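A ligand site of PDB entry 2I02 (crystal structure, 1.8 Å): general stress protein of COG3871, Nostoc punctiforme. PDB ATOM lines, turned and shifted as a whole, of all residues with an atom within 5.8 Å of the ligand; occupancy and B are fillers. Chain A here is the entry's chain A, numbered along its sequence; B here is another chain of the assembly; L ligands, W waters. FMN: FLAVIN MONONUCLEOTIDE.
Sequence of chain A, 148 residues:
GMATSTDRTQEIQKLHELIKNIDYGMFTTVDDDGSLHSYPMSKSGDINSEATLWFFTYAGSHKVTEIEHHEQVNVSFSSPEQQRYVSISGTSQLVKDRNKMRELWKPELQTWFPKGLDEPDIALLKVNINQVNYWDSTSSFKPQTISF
N of Lys 63 is in hydrogen-bond range of O1P of the ligand, 2.8 Å away.
NZ of Lys 63 lies within salt-bridge range of O1P of the ligand, at 2.6 Å.
The backbone carbonyl oxygen (O) of Phe 141 of chain B is in hydrogen-bond range of an oxygen (O3') of the ligand (2.7 Å).
The backbone carbonyl oxygen of Phe 56 sits at hydrogen-bond distance from a nitrogen (N3) of the ligand (2.8 Å).
An oxygen (O2') of the ligand is in hydrogen-bond range of the backbone carbonyl oxygen of Pro 40, 2.8 Å away.
The indole nitrogen (NE1) of Trp 135 of chain B is in hydrogen-bond range of an oxygen (O3') of the ligand, 3.1 Å away.
The backbone NH (N) of His 62 lies within hydrogen-bond range of an oxygen (O2P) of the ligand (3.2 Å).
The backbone NH (N) of Ser 42 is in hydrogen-bond range of an oxygen (O4) of the ligand, at 3.3 Å.
An oxygen (O2) of the ligand is in hydrogen-bond range of the side-chain hydroxyl of Thr 57, 3.4 Å away.
The side-chain sulfur (SD) of Met 41 lies close to a nitrogen (N3) of the ligand (3.5 Å).
The indole nitrogen of Trp 135 of chain B sits at hydrogen-bond distance from the backbone carbonyl oxygen of Phe 141 of chain B (2.7 Å).
The backbone NH (N) of Trp 135 of chain B sits at hydrogen-bond distance from the backbone carbonyl oxygen (O) of Tyr 85 of chain B, 2.9 Å away.
A ring nitrogen (NE2) of His 62 lies close to the side-chain carboxylate of Glu 66 (3.1 Å).
The backbone carbonyl oxygen (O) of Trp 112 is in hydrogen-bond range of the side-chain hydroxyl (OH) of Tyr 58, 2.7 Å away.
The side-chain hydroxyl of Thr 57 sits at hydrogen-bond distance from the side-chain hydroxyl of Ser 61, at 3.5 Å.
OE1 of Glu 66 lies within hydrogen-bond range of OH of Tyr 39, 2.8 Å away.
OG of Ser 61 lies within hydrogen-bond range of O of Tyr 58, at 2.8 Å.
Tyr 24 touches the ligand.
Tyr 39 touches the ligand (CE2 to O3P, 3.4 Å).
Ser 61 touches the ligand (CB to O1P, 3.4 Å).
CZ2 of Trp 112 touches C6 of the ligand, 3.2 Å away.
CZ of Phe 113 touches N3 of the ligand (3.7 Å).
CE2 of Tyr 85 of chain B touches C7M of the ligand, 3.9 Å away.
Pro 143 of chain B touches the ligand (CD to O3', 3.8 Å).
Hydrophobic or aromatic side chains that line the ligand: Tyr 24, Tyr 39, Pro 40, Met 41, His 62, Trp 112, Phe 113, Tyr 85 of chain B, Trp 135 of chain B, Phe 141 of chain B and Pro 143 of chain B.
Of the 24 residues printed, 16 come within 4 Å of the ligand.
Along chain A the residues within 4 Å of the ligand span positions 24 to 113.
Water W2 lies within hydrogen-bond range of an oxygen (O4) of the ligand (2.5 Å), the backbone carbonyl oxygen of Ser 42 (2.8 Å) and the backbone NH of Phe 56 (2.8 Å).
Water W3 lies within hydrogen-bond range of O2 of the ligand (2.7 Å), NZ of Lys 63 (3.1 Å), OG1 of Thr 57 (3.4 Å) and N of Tyr 58 (3.5 Å).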
ATOM      1  N   TYR A  24     -30.350  12.000 -16.509  1.00  0.00           N
ATOM      2  CA  TYR A  24     -29.919  12.749 -15.325  1.00  0.00           C
ATOM      3  C   TYR A  24     -29.885  14.240 -15.699  1.00  0.00           C
ATOM      4  O   TYR A  24     -29.421  14.607 -16.755  1.00  0.00           O
ATOM      5  CB  TYR A  24     -28.546  12.296 -14.808  1.00  0.00           C
ATOM      6  CG  TYR A  24     -28.435  10.795 -14.599  1.00  0.00           C
ATOM      7  CD1 TYR A  24     -29.156  10.160 -13.597  1.00  0.00           C
ATOM      8  CD2 TYR A  24     -27.676  10.000 -15.457  1.00  0.00           C
ATOM      9  CE1 TYR A  24     -29.090   8.779 -13.425  1.00  0.00           C
ATOM     10  CE2 TYR A  24     -27.611   8.630 -15.306  1.00  0.00           C
ATOM     11  CZ  TYR A  24     -28.319   8.023 -14.286  1.00  0.00           C
ATOM     12  OH  TYR A  24     -28.252   6.642 -14.113  1.00  0.00           O
ATOM     13  N   TYR A  39     -26.245  19.374  -8.404  1.00  0.00           N
ATOM     14  CA  TYR A  39     -26.283  17.970  -8.035  1.00  0.00           C
ATOM     15  C   TYR A  39     -26.903  17.145  -9.160  1.00  0.00           C
ATOM     16  O   TYR A  39     -27.966  17.516  -9.634  1.00  0.00           O
ATOM     17  CB  TYR A  39     -27.220  17.790  -6.819  1.00  0.00           C
ATOM     18  CG  TYR A  39     -27.024  18.722  -5.670  1.00  0.00           C
ATOM     19  CD1 TYR A  39     -27.670  19.954  -5.601  1.00  0.00           C
ATOM     20  CD2 TYR A  39     -26.252  18.342  -4.576  1.00  0.00           C
ATOM     21  CE1 TYR A  39     -27.474  20.809  -4.519  1.00  0.00           C
ATOM     22  CE2 TYR A  39     -26.067  19.181  -3.483  1.00  0.00           C
ATOM     23  CZ  TYR A  39     -26.676  20.414  -3.448  1.00  0.00           C
ATOM     24  OH  TYR A  39     -26.474  21.217  -2.325  1.00  0.00           O
ATOM     25  N   PRO A  40     -26.302  16.014  -9.533  1.00  0.00           N
ATOM     26  CA  PRO A  40     -26.987  15.155 -10.511  1.00  0.00           C
ATOM     27  C   PRO A  40     -28.211  14.514  -9.906  1.00  0.00           C
ATOM     28  O   PRO A  40     -28.159  14.079  -8.777  1.00  0.00           O
ATOM     29  CB  PRO A  40     -25.955  14.102 -10.886  1.00  0.00           C
ATOM     30  CG  PRO A  40     -24.998  14.091  -9.788  1.00  0.00           C
ATOM     31  CD  PRO A  40     -25.013  15.441  -9.124  1.00  0.00           C
ATOM     32  N   MET A  41     -29.301  14.492 -10.651  1.00  0.00           N
ATOM     33  CA  MET A  41     -30.567  13.941 -10.173  1.00  0.00           C
ATOM     34  C   MET A  41     -31.228  13.150 -11.291  1.00  0.00           C
ATOM     35  O   MET A  41     -31.264  13.601 -12.418  1.00  0.00           O
ATOM     36  CB  MET A  41     -31.507  15.066  -9.714  1.00  0.00           C
ATOM     37  CG  MET A  41     -30.997  15.927  -8.569  1.00  0.00           C
ATOM     38  SD  MET A  41     -30.788  14.971  -6.894  1.00  0.00           S
ATOM     39  CE  MET A  41     -32.597  15.126  -6.214  1.00  0.00           C
ATOM     40  N   SER A  42     -31.757  11.981 -10.957  1.00  0.00           N
ATOM     41  CA  SER A  42     -32.471  11.160 -11.919  1.00  0.00           C
ATOM     42  C   SER A  42     -33.910  11.631 -11.998  1.00  0.00           C
ATOM     43  O   SER A  42     -34.574  11.646 -11.001  1.00  0.00           O
ATOM     44  CB  SER A  42     -32.443   9.693 -11.453  1.00  0.00           C
ATOM     45  OG  SER A  42     -32.996   8.858 -12.458  1.00  0.00           O
ATOM     46  N   PHE A  55     -38.450  14.537  -8.620  1.00  0.00           N
ATOM     47  CA  PHE A  55     -37.218  13.806  -8.262  1.00  0.00           C
ATOM     48  C   PHE A  55     -37.377  13.233  -6.874  1.00  0.00           C
ATOM     49  O   PHE A  55     -37.970  13.888  -6.011  1.00  0.00           O
ATOM     50  CB  PHE A  55     -36.000  14.737  -8.239  1.00  0.00           C
ATOM     51  CG  PHE A  55     -35.790  15.493  -9.507  1.00  0.00           C
ATOM     52  CD1 PHE A  55     -36.419  16.711  -9.718  1.00  0.00           C
ATOM     53  CD2 PHE A  55     -34.970  14.978 -10.500  1.00  0.00           C
ATOM     54  CE1 PHE A  55     -36.239  17.426 -10.932  1.00  0.00           C
ATOM     55  CE2 PHE A  55     -34.761  15.672 -11.694  1.00  0.00           C
ATOM     56  CZ  PHE A  55     -35.406  16.874 -11.908  1.00  0.00           C
ATOM     57  N   PHE A  56     -36.846  12.038  -6.669  1.00  0.00           N
ATOM     58  CA  PHE A  56     -36.724  11.496  -5.319  1.00  0.00           C
ATOM     59  C   PHE A  56     -35.515  12.096  -4.628  1.00  0.00           C
ATOM     60  O   PHE A  56     -34.475  12.332  -5.260  1.00  0.00           O
ATOM     61  CB  PHE A  56     -36.612   9.964  -5.392  1.00  0.00           C
ATOM     62  CG  PHE A  56     -37.913   9.287  -5.639  1.00  0.00           C
ATOM     63  CD1 PHE A  56     -38.737   8.880  -4.587  1.00  0.00           C
ATOM     64  CD2 PHE A  56     -38.310   8.996  -6.948  1.00  0.00           C
ATOM     65  CE1 PHE A  56     -39.928   8.226  -4.824  1.00  0.00           C
ATOM     66  CE2 PHE A  56     -39.513   8.360  -7.188  1.00  0.00           C
ATOM     67  CZ  PHE A  56     -40.325   7.964  -6.118  1.00  0.00           C
ATOM     68  N   THR A  57     -35.641  12.377  -3.332  1.00  0.00           N
ATOM     69  CA  THR A  57     -34.546  12.906  -2.524  1.00  0.00           C
ATOM     70  C   THR A  57     -34.683  12.367  -1.083  1.00  0.00           C
ATOM     71  O   THR A  57     -35.615  11.603  -0.803  1.00  0.00           O
ATOM     72  CB  THR A  57     -34.535  14.417  -2.519  1.00  0.00           C
ATOM     73  OG1 THR A  57     -33.268  14.865  -2.034  1.00  0.00           O
ATOM     74  CG2 THR A  57     -35.699  14.991  -1.684  1.00  0.00           C
ATOM     75  N   TYR A  58     -33.732  12.699  -0.217  1.00  0.00           N
ATOM     76  CA  TYR A  58     -33.848  12.436   1.226  1.00  0.00           C
ATOM     77  C   TYR A  58     -34.270  13.769   1.849  1.00  0.00           C
ATOM     78  O   TYR A  58     -33.692  14.816   1.528  1.00  0.00           O
ATOM     79  CB  TYR A  58     -32.540  11.930   1.815  1.00  0.00           C
ATOM     80  CG  TYR A  58     -32.173  10.555   1.321  1.00  0.00           C
ATOM     81  CD1 TYR A  58     -32.785   9.436   1.860  1.00  0.00           C
ATOM     82  CD2 TYR A  58     -31.241  10.381   0.318  1.00  0.00           C
ATOM     83  CE1 TYR A  58     -32.455   8.154   1.416  1.00  0.00           C
ATOM     84  CE2 TYR A  58     -30.911   9.104  -0.156  1.00  0.00           C
ATOM     85  CZ  TYR A  58     -31.518   8.008   0.404  1.00  0.00           C
ATOM     86  OH  TYR A  58     -31.199   6.734  -0.022  1.00  0.00           O
ATOM     87  N   GLY A  60     -33.877  14.944   4.726  1.00  0.00           N
ATOM     88  CA  GLY A  60     -32.826  15.559   5.512  1.00  0.00           C
ATOM     89  C   GLY A  60     -31.624  16.064   4.742  1.00  0.00           C
ATOM     90  O   GLY A  60     -30.669  16.523   5.356  1.00  0.00           O
ATOM     91  N   SER A  61     -31.650  15.985   3.406  1.00  0.00           N
ATOM     92  CA  SER A  61     -30.545  16.418   2.577  1.00  0.00           C
ATOM     93  C   SER A  61     -30.307  17.944   2.614  1.00  0.00           C
ATOM     94  O   SER A  61     -31.210  18.747   2.909  1.00  0.00           O
ATOM     95  CB  SER A  61     -30.751  15.985   1.125  1.00  0.00           C
ATOM     96  OG  SER A  61     -31.846  16.671   0.552  1.00  0.00           O
ATOM     97  N   HIS A  62     -29.083  18.330   2.311  1.00  0.00           N
ATOM     98  CA  HIS A  62     -28.738  19.745   2.334  1.00  0.00           C
ATOM     99  C   HIS A  62     -29.515  20.491   1.246  1.00  0.00           C
ATOM    100  O   HIS A  62     -29.946  21.599   1.468  1.00  0.00           O
ATOM    101  CB  HIS A  62     -27.210  19.955   2.185  1.00  0.00           C
ATOM    102  CG  HIS A  62     -26.807  21.385   2.383  1.00  0.00           C
ATOM    103  ND1 HIS A  62     -27.040  22.064   3.569  1.00  0.00           N
ATOM    104  CD2 HIS A  62     -26.208  22.265   1.556  1.00  0.00           C
ATOM    105  CE1 HIS A  62     -26.616  23.303   3.447  1.00  0.00           C
ATOM    106  NE2 HIS A  62     -26.100  23.457   2.246  1.00  0.00           N
ATOM    107  N   LYS A  63     -29.738  19.893   0.086  1.00  0.00           N
ATOM    108  CA  LYS A  63     -30.478  20.567  -0.978  1.00  0.00           C
ATOM    109  C   LYS A  63     -31.898  20.939  -0.530  1.00  0.00           C
ATOM    110  O   LYS A  63     -32.461  21.922  -0.957  1.00  0.00           O
ATOM    111  CB  LYS A  63     -30.495  19.755  -2.287  1.00  0.00           C
ATOM    112  CG  LYS A  63     -31.394  18.509  -2.325  1.00  0.00           C
ATOM    113  CD  LYS A  63     -31.242  17.753  -3.642  1.00  0.00           C
ATOM    114  CE  LYS A  63     -29.909  16.976  -3.733  1.00  0.00           C
ATOM    115  NZ  LYS A  63     -29.791  16.057  -2.548  1.00  0.00           N
ATOM    116  N   VAL A  64     -32.498  20.118   0.327  1.00  0.00           N
ATOM    117  CA  VAL A  64     -33.824  20.423   0.840  1.00  0.00           C
ATOM    118  C   VAL A  64     -33.790  21.623   1.769  1.00  0.00           C
ATOM    119  O   VAL A  64     -34.644  22.505   1.716  1.00  0.00           O
ATOM    120  CB  VAL A  64     -34.461  19.136   1.534  1.00  0.00           C
ATOM    121  CG1 VAL A  64     -35.685  19.512   2.312  1.00  0.00           C
ATOM    122  CG2 VAL A  64     -34.796  18.089   0.495  1.00  0.00           C
ATOM    123  N   GLU A  66     -31.692  24.008   1.461  1.00  0.00           N
ATOM    124  CA  GLU A  66     -31.550  25.148   0.560  1.00  0.00           C
ATOM    125  C   GLU A  66     -32.877  25.570  -0.016  1.00  0.00           C
ATOM    126  O   GLU A  66     -33.232  26.768   0.005  1.00  0.00           O
ATOM    127  CB  GLU A  66     -30.502  24.842  -0.541  1.00  0.00           C
ATOM    128  CG  GLU A  66     -29.125  24.561   0.073  1.00  0.00           C
ATOM    129  CD  GLU A  66     -28.070  23.944  -0.847  1.00  0.00           C
ATOM    130  OE1 GLU A  66     -28.390  23.143  -1.771  1.00  0.00           O
ATOM    131  OE2 GLU A  66     -26.873  24.255  -0.609  1.00  0.00           O
ATOM    132  N   LEU A 109     -33.909   3.429  -9.330  1.00  0.00           N
ATOM    133  CA  LEU A 109     -33.620   4.354  -8.240  1.00  0.00           C
ATOM    134  C   LEU A 109     -33.031   3.668  -6.994  1.00  0.00           C
ATOM    135  O   LEU A 109     -32.520   4.342  -6.111  1.00  0.00           O
ATOM    136  CB  LEU A 109     -34.881   5.119  -7.861  1.00  0.00           C
ATOM    137  CG  LEU A 109     -35.327   6.101  -8.949  1.00  0.00           C
ATOM    138  CD1 LEU A 109     -36.619   6.772  -8.539  1.00  0.00           C
ATOM    139  CD2 LEU A 109     -34.255   7.139  -9.234  1.00  0.00           C
ATOM    140  N   TRP A 112     -29.588   4.747  -5.569  1.00  0.00           N
ATOM    141  CA  TRP A 112     -29.408   5.844  -4.628  1.00  0.00           C
ATOM    142  C   TRP A 112     -30.330   5.714  -3.424  1.00  0.00           C
ATOM    143  O   TRP A 112     -30.143   6.427  -2.438  1.00  0.00           O
ATOM    144  CB  TRP A 112     -29.602   7.208  -5.317  1.00  0.00           C
ATOM    145  CG  TRP A 112     -28.686   7.340  -6.460  1.00  0.00           C
ATOM    146  CD1 TRP A 112     -27.371   7.708  -6.429  1.00  0.00           C
ATOM    147  CD2 TRP A 112     -28.981   7.013  -7.816  1.00  0.00           C
ATOM    148  NE1 TRP A 112     -26.835   7.648  -7.690  1.00  0.00           N
ATOM    149  CE2 TRP A 112     -27.795   7.224  -8.562  1.00  0.00           C
ATOM    150  CE3 TRP A 112     -30.126   6.586  -8.481  1.00  0.00           C
ATOM    151  CZ2 TRP A 112     -27.741   7.007  -9.932  1.00  0.00           C
ATOM    152  CZ3 TRP A 112     -30.063   6.375  -9.853  1.00  0.00           C
ATOM    153  CH2 TRP A 112     -28.884   6.593 -10.567  1.00  0.00           C
ATOM    154  N   PHE A 113     -31.309   4.800  -3.531  1.00  0.00           N
ATOM    155  CA  PHE A 113     -32.322   4.513  -2.485  1.00  0.00           C
ATOM    156  C   PHE A 113     -32.437   3.004  -2.248  1.00  0.00           C
ATOM    157  O   PHE A 113     -33.394   2.352  -2.686  1.00  0.00           O
ATOM    158  CB  PHE A 113     -33.681   5.130  -2.885  1.00  0.00           C
ATOM    159  CG  PHE A 113     -33.611   6.604  -3.100  1.00  0.00           C
ATOM    160  CD1 PHE A 113     -33.722   7.482  -2.040  1.00  0.00           C
ATOM    161  CD2 PHE A 113     -33.417   7.136  -4.373  1.00  0.00           C
ATOM    162  CE1 PHE A 113     -33.623   8.855  -2.235  1.00  0.00           C
ATOM    163  CE2 PHE A 113     -33.334   8.493  -4.571  1.00  0.00           C
ATOM    164  CZ  PHE A 113     -33.433   9.352  -3.507  1.00  0.00           C
ATOM    165  N   TYR B  85     -19.923  13.615 -13.468  1.00  0.00           N
ATOM    166  CA  TYR B  85     -20.704  14.822 -13.192  1.00  0.00           C
ATOM    167  C   TYR B  85     -19.886  15.740 -12.293  1.00  0.00           C
ATOM    168  O   TYR B  85     -19.280  15.283 -11.340  1.00  0.00           O
ATOM    169  CB  TYR B  85     -22.035  14.475 -12.551  1.00  0.00           C
ATOM    170  CG  TYR B  85     -22.706  13.403 -13.335  1.00  0.00           C
ATOM    171  CD1 TYR B  85     -23.465  13.722 -14.456  1.00  0.00           C
ATOM    172  CD2 TYR B  85     -22.446  12.073 -13.060  1.00  0.00           C
ATOM    173  CE1 TYR B  85     -24.018  12.713 -15.248  1.00  0.00           C
ATOM    174  CE2 TYR B  85     -23.003  11.052 -13.844  1.00  0.00           C
ATOM    175  CZ  TYR B  85     -23.782  11.386 -14.928  1.00  0.00           C
ATOM    176  OH  TYR B  85     -24.304  10.374 -15.700  1.00  0.00           O
ATOM    177  N   TRP B 135     -18.860  13.586  -9.042  1.00  0.00           N
ATOM    178  CA  TRP B 135     -19.337  12.219  -8.942  1.00  0.00           C
ATOM    179  C   TRP B 135     -18.763  11.460 -10.096  1.00  0.00           C
ATOM    180  O   TRP B 135     -18.954  11.830 -11.256  1.00  0.00           O
ATOM    181  CB  TRP B 135     -20.864  12.223  -9.050  1.00  0.00           C
ATOM    182  CG  TRP B 135     -21.594  13.005  -7.935  1.00  0.00           C
ATOM    183  CD1 TRP B 135     -22.245  12.463  -6.843  1.00  0.00           C
ATOM    184  CD2 TRP B 135     -21.773  14.411  -7.849  1.00  0.00           C
ATOM    185  NE1 TRP B 135     -22.786  13.475  -6.075  1.00  0.00           N
ATOM    186  CE2 TRP B 135     -22.542  14.681  -6.682  1.00  0.00           C
ATOM    187  CE3 TRP B 135     -21.350  15.499  -8.633  1.00  0.00           C
ATOM    188  CZ2 TRP B 135     -22.855  15.978  -6.272  1.00  0.00           C
ATOM    189  CZ3 TRP B 135     -21.694  16.787  -8.221  1.00  0.00           C
ATOM    190  CH2 TRP B 135     -22.432  17.001  -7.057  1.00  0.00           C
ATOM    191  N   SER B 140     -20.149   7.934  -7.221  1.00  0.00           N
ATOM    192  CA  SER B 140     -21.589   8.177  -7.110  1.00  0.00           C
ATOM    193  C   SER B 140     -22.009   8.658  -5.703  1.00  0.00           C
ATOM    194  O   SER B 140     -21.144   8.970  -4.884  1.00  0.00           O
ATOM    195  CB  SER B 140     -22.367   6.929  -7.566  1.00  0.00           C
ATOM    196  OG  SER B 140     -22.395   5.918  -6.558  1.00  0.00           O
ATOM    197  N   PHE B 141     -23.325   8.624  -5.434  1.00  0.00           N
ATOM    198  CA  PHE B 141     -24.061   9.422  -4.383  1.00  0.00           C
ATOM    199  C   PHE B 141     -23.413  10.701  -3.753  1.00  0.00           C
ATOM    200  O   PHE B 141     -23.729  11.813  -4.183  1.00  0.00           O
ATOM    201  CB  PHE B 141     -24.652   8.566  -3.255  1.00  0.00           C
ATOM    202  CG  PHE B 141     -25.723   9.309  -2.462  1.00  0.00           C
ATOM    203  CD1 PHE B 141     -26.973   9.577  -3.034  1.00  0.00           C
ATOM    204  CD2 PHE B 141     -25.461   9.783  -1.175  1.00  0.00           C
ATOM    205  CE1 PHE B 141     -27.964  10.279  -2.326  1.00  0.00           C
ATOM    206  CE2 PHE B 141     -26.440  10.490  -0.456  1.00  0.00           C
ATOM    207  CZ  PHE B 141     -27.695  10.741  -1.042  1.00  0.00           C
ATOM    208  N   LYS B 142     -22.599  10.560  -2.699  1.00  0.00           N
ATOM    209  CA  LYS B 142     -21.906  11.733  -2.158  1.00  0.00           C
ATOM    210  C   LYS B 142     -20.788  12.121  -3.103  1.00  0.00           C
ATOM    211  O   LYS B 142     -20.107  11.266  -3.669  1.00  0.00           O
ATOM    212  CB  LYS B 142     -21.341  11.490  -0.752  1.00  0.00           C
ATOM    213  N   PRO B 143     -20.614  13.438  -3.308  1.00  0.00           N
ATOM    214  CA  PRO B 143     -19.530  13.809  -4.168  1.00  0.00           C
ATOM    215  C   PRO B 143     -18.231  13.702  -3.446  1.00  0.00           C
ATOM    216  O   PRO B 143     -18.183  13.524  -2.239  1.00  0.00           O
ATOM    217  CB  PRO B 143     -19.799  15.291  -4.460  1.00  0.00           C
ATOM    218  CG  PRO B 143     -20.538  15.780  -3.219  1.00  0.00           C
ATOM    219  CD  PRO B 143     -21.382  14.591  -2.822  1.00  0.00           C
HETATM  220  N1  FMN L   1     -29.501  12.181  -5.002  1.00  0.00           N
HETATM  221  C2  FMN L   1     -30.824  12.273  -4.640  1.00  0.00           C
HETATM  222  O2  FMN L   1     -31.116  12.743  -3.489  1.00  0.00           O
HETATM  223  N3  FMN L   1     -31.766  11.856  -5.591  1.00  0.00           N
HETATM  224  C4  FMN L   1     -31.398  11.373  -6.863  1.00  0.00           C
HETATM  225  O4  FMN L   1     -32.235  11.224  -7.793  1.00  0.00           O
HETATM  226  C4A FMN L   1     -30.055  11.263  -7.195  1.00  0.00           C
HETATM  227  N5  FMN L   1     -29.643  10.782  -8.436  1.00  0.00           N
HETATM  228  C5A FMN L   1     -28.271  10.716  -8.709  1.00  0.00           C
HETATM  229  C6  FMN L   1     -27.864  10.241  -9.956  1.00  0.00           C
HETATM  230  C7  FMN L   1     -26.504  10.170 -10.277  1.00  0.00           C
HETATM  231  C7M FMN L   1     -26.112  10.127 -11.738  1.00  0.00           C
HETATM  232  C8  FMN L   1     -25.561  10.546  -9.319  1.00  0.00           C
HETATM  233  C8M FMN L   1     -24.109  10.586  -9.639  1.00  0.00           C
HETATM  234  C9  FMN L   1     -25.963  11.014  -8.066  1.00  0.00           C
HETATM  235  C9A FMN L   1     -27.310  11.125  -7.749  1.00  0.00           C
HETATM  236  N10 FMN L   1     -27.745  11.637  -6.522  1.00  0.00           N
HETATM  237  C10 FMN L   1     -29.108  11.673  -6.237  1.00  0.00           C
HETATM  238  C1' FMN L   1     -26.869  12.268  -5.466  1.00  0.00           C
HETATM  239  C2' FMN L   1     -26.985  13.805  -5.436  1.00  0.00           C
HETATM  240  O2' FMN L   1     -26.333  14.258  -6.610  1.00  0.00           O
HETATM  241  C3' FMN L   1     -26.403  14.406  -4.153  1.00  0.00           C
HETATM  242  O3' FMN L   1     -24.978  14.195  -3.947  1.00  0.00           O
HETATM  243  C4' FMN L   1     -27.047  13.798  -2.893  1.00  0.00           C
HETATM  244  O4' FMN L   1     -28.461  13.795  -2.956  1.00  0.00           O
HETATM  245  C5' FMN L   1     -26.635  14.545  -1.622  1.00  0.00           C
HETATM  246  O5' FMN L   1     -26.964  15.893  -1.778  1.00  0.00           O
HETATM  247  P   FMN L   1     -27.190  16.853  -0.517  1.00  0.00           P
HETATM  248  O1P FMN L   1     -28.437  17.562  -0.885  1.00  0.00           O
HETATM  249  O2P FMN L   1     -27.273  16.112   0.808  1.00  0.00           O
HETATM  250  O3P FMN L   1     -26.021  17.827  -0.381  1.00  0.00           O
HETATM  251  O   HOH W   1     -28.671  13.432   1.328  1.00  0.00           O
HETATM  252  O   HOH W   2     -34.673  11.073  -8.237  1.00  0.00           O
HETATM  253  O   HOH W   3     -30.397  13.395  -0.987  1.00  0.00           O
HETATM  254  O   HOH W   4     -23.691  16.774  -2.638  1.00  0.00           O
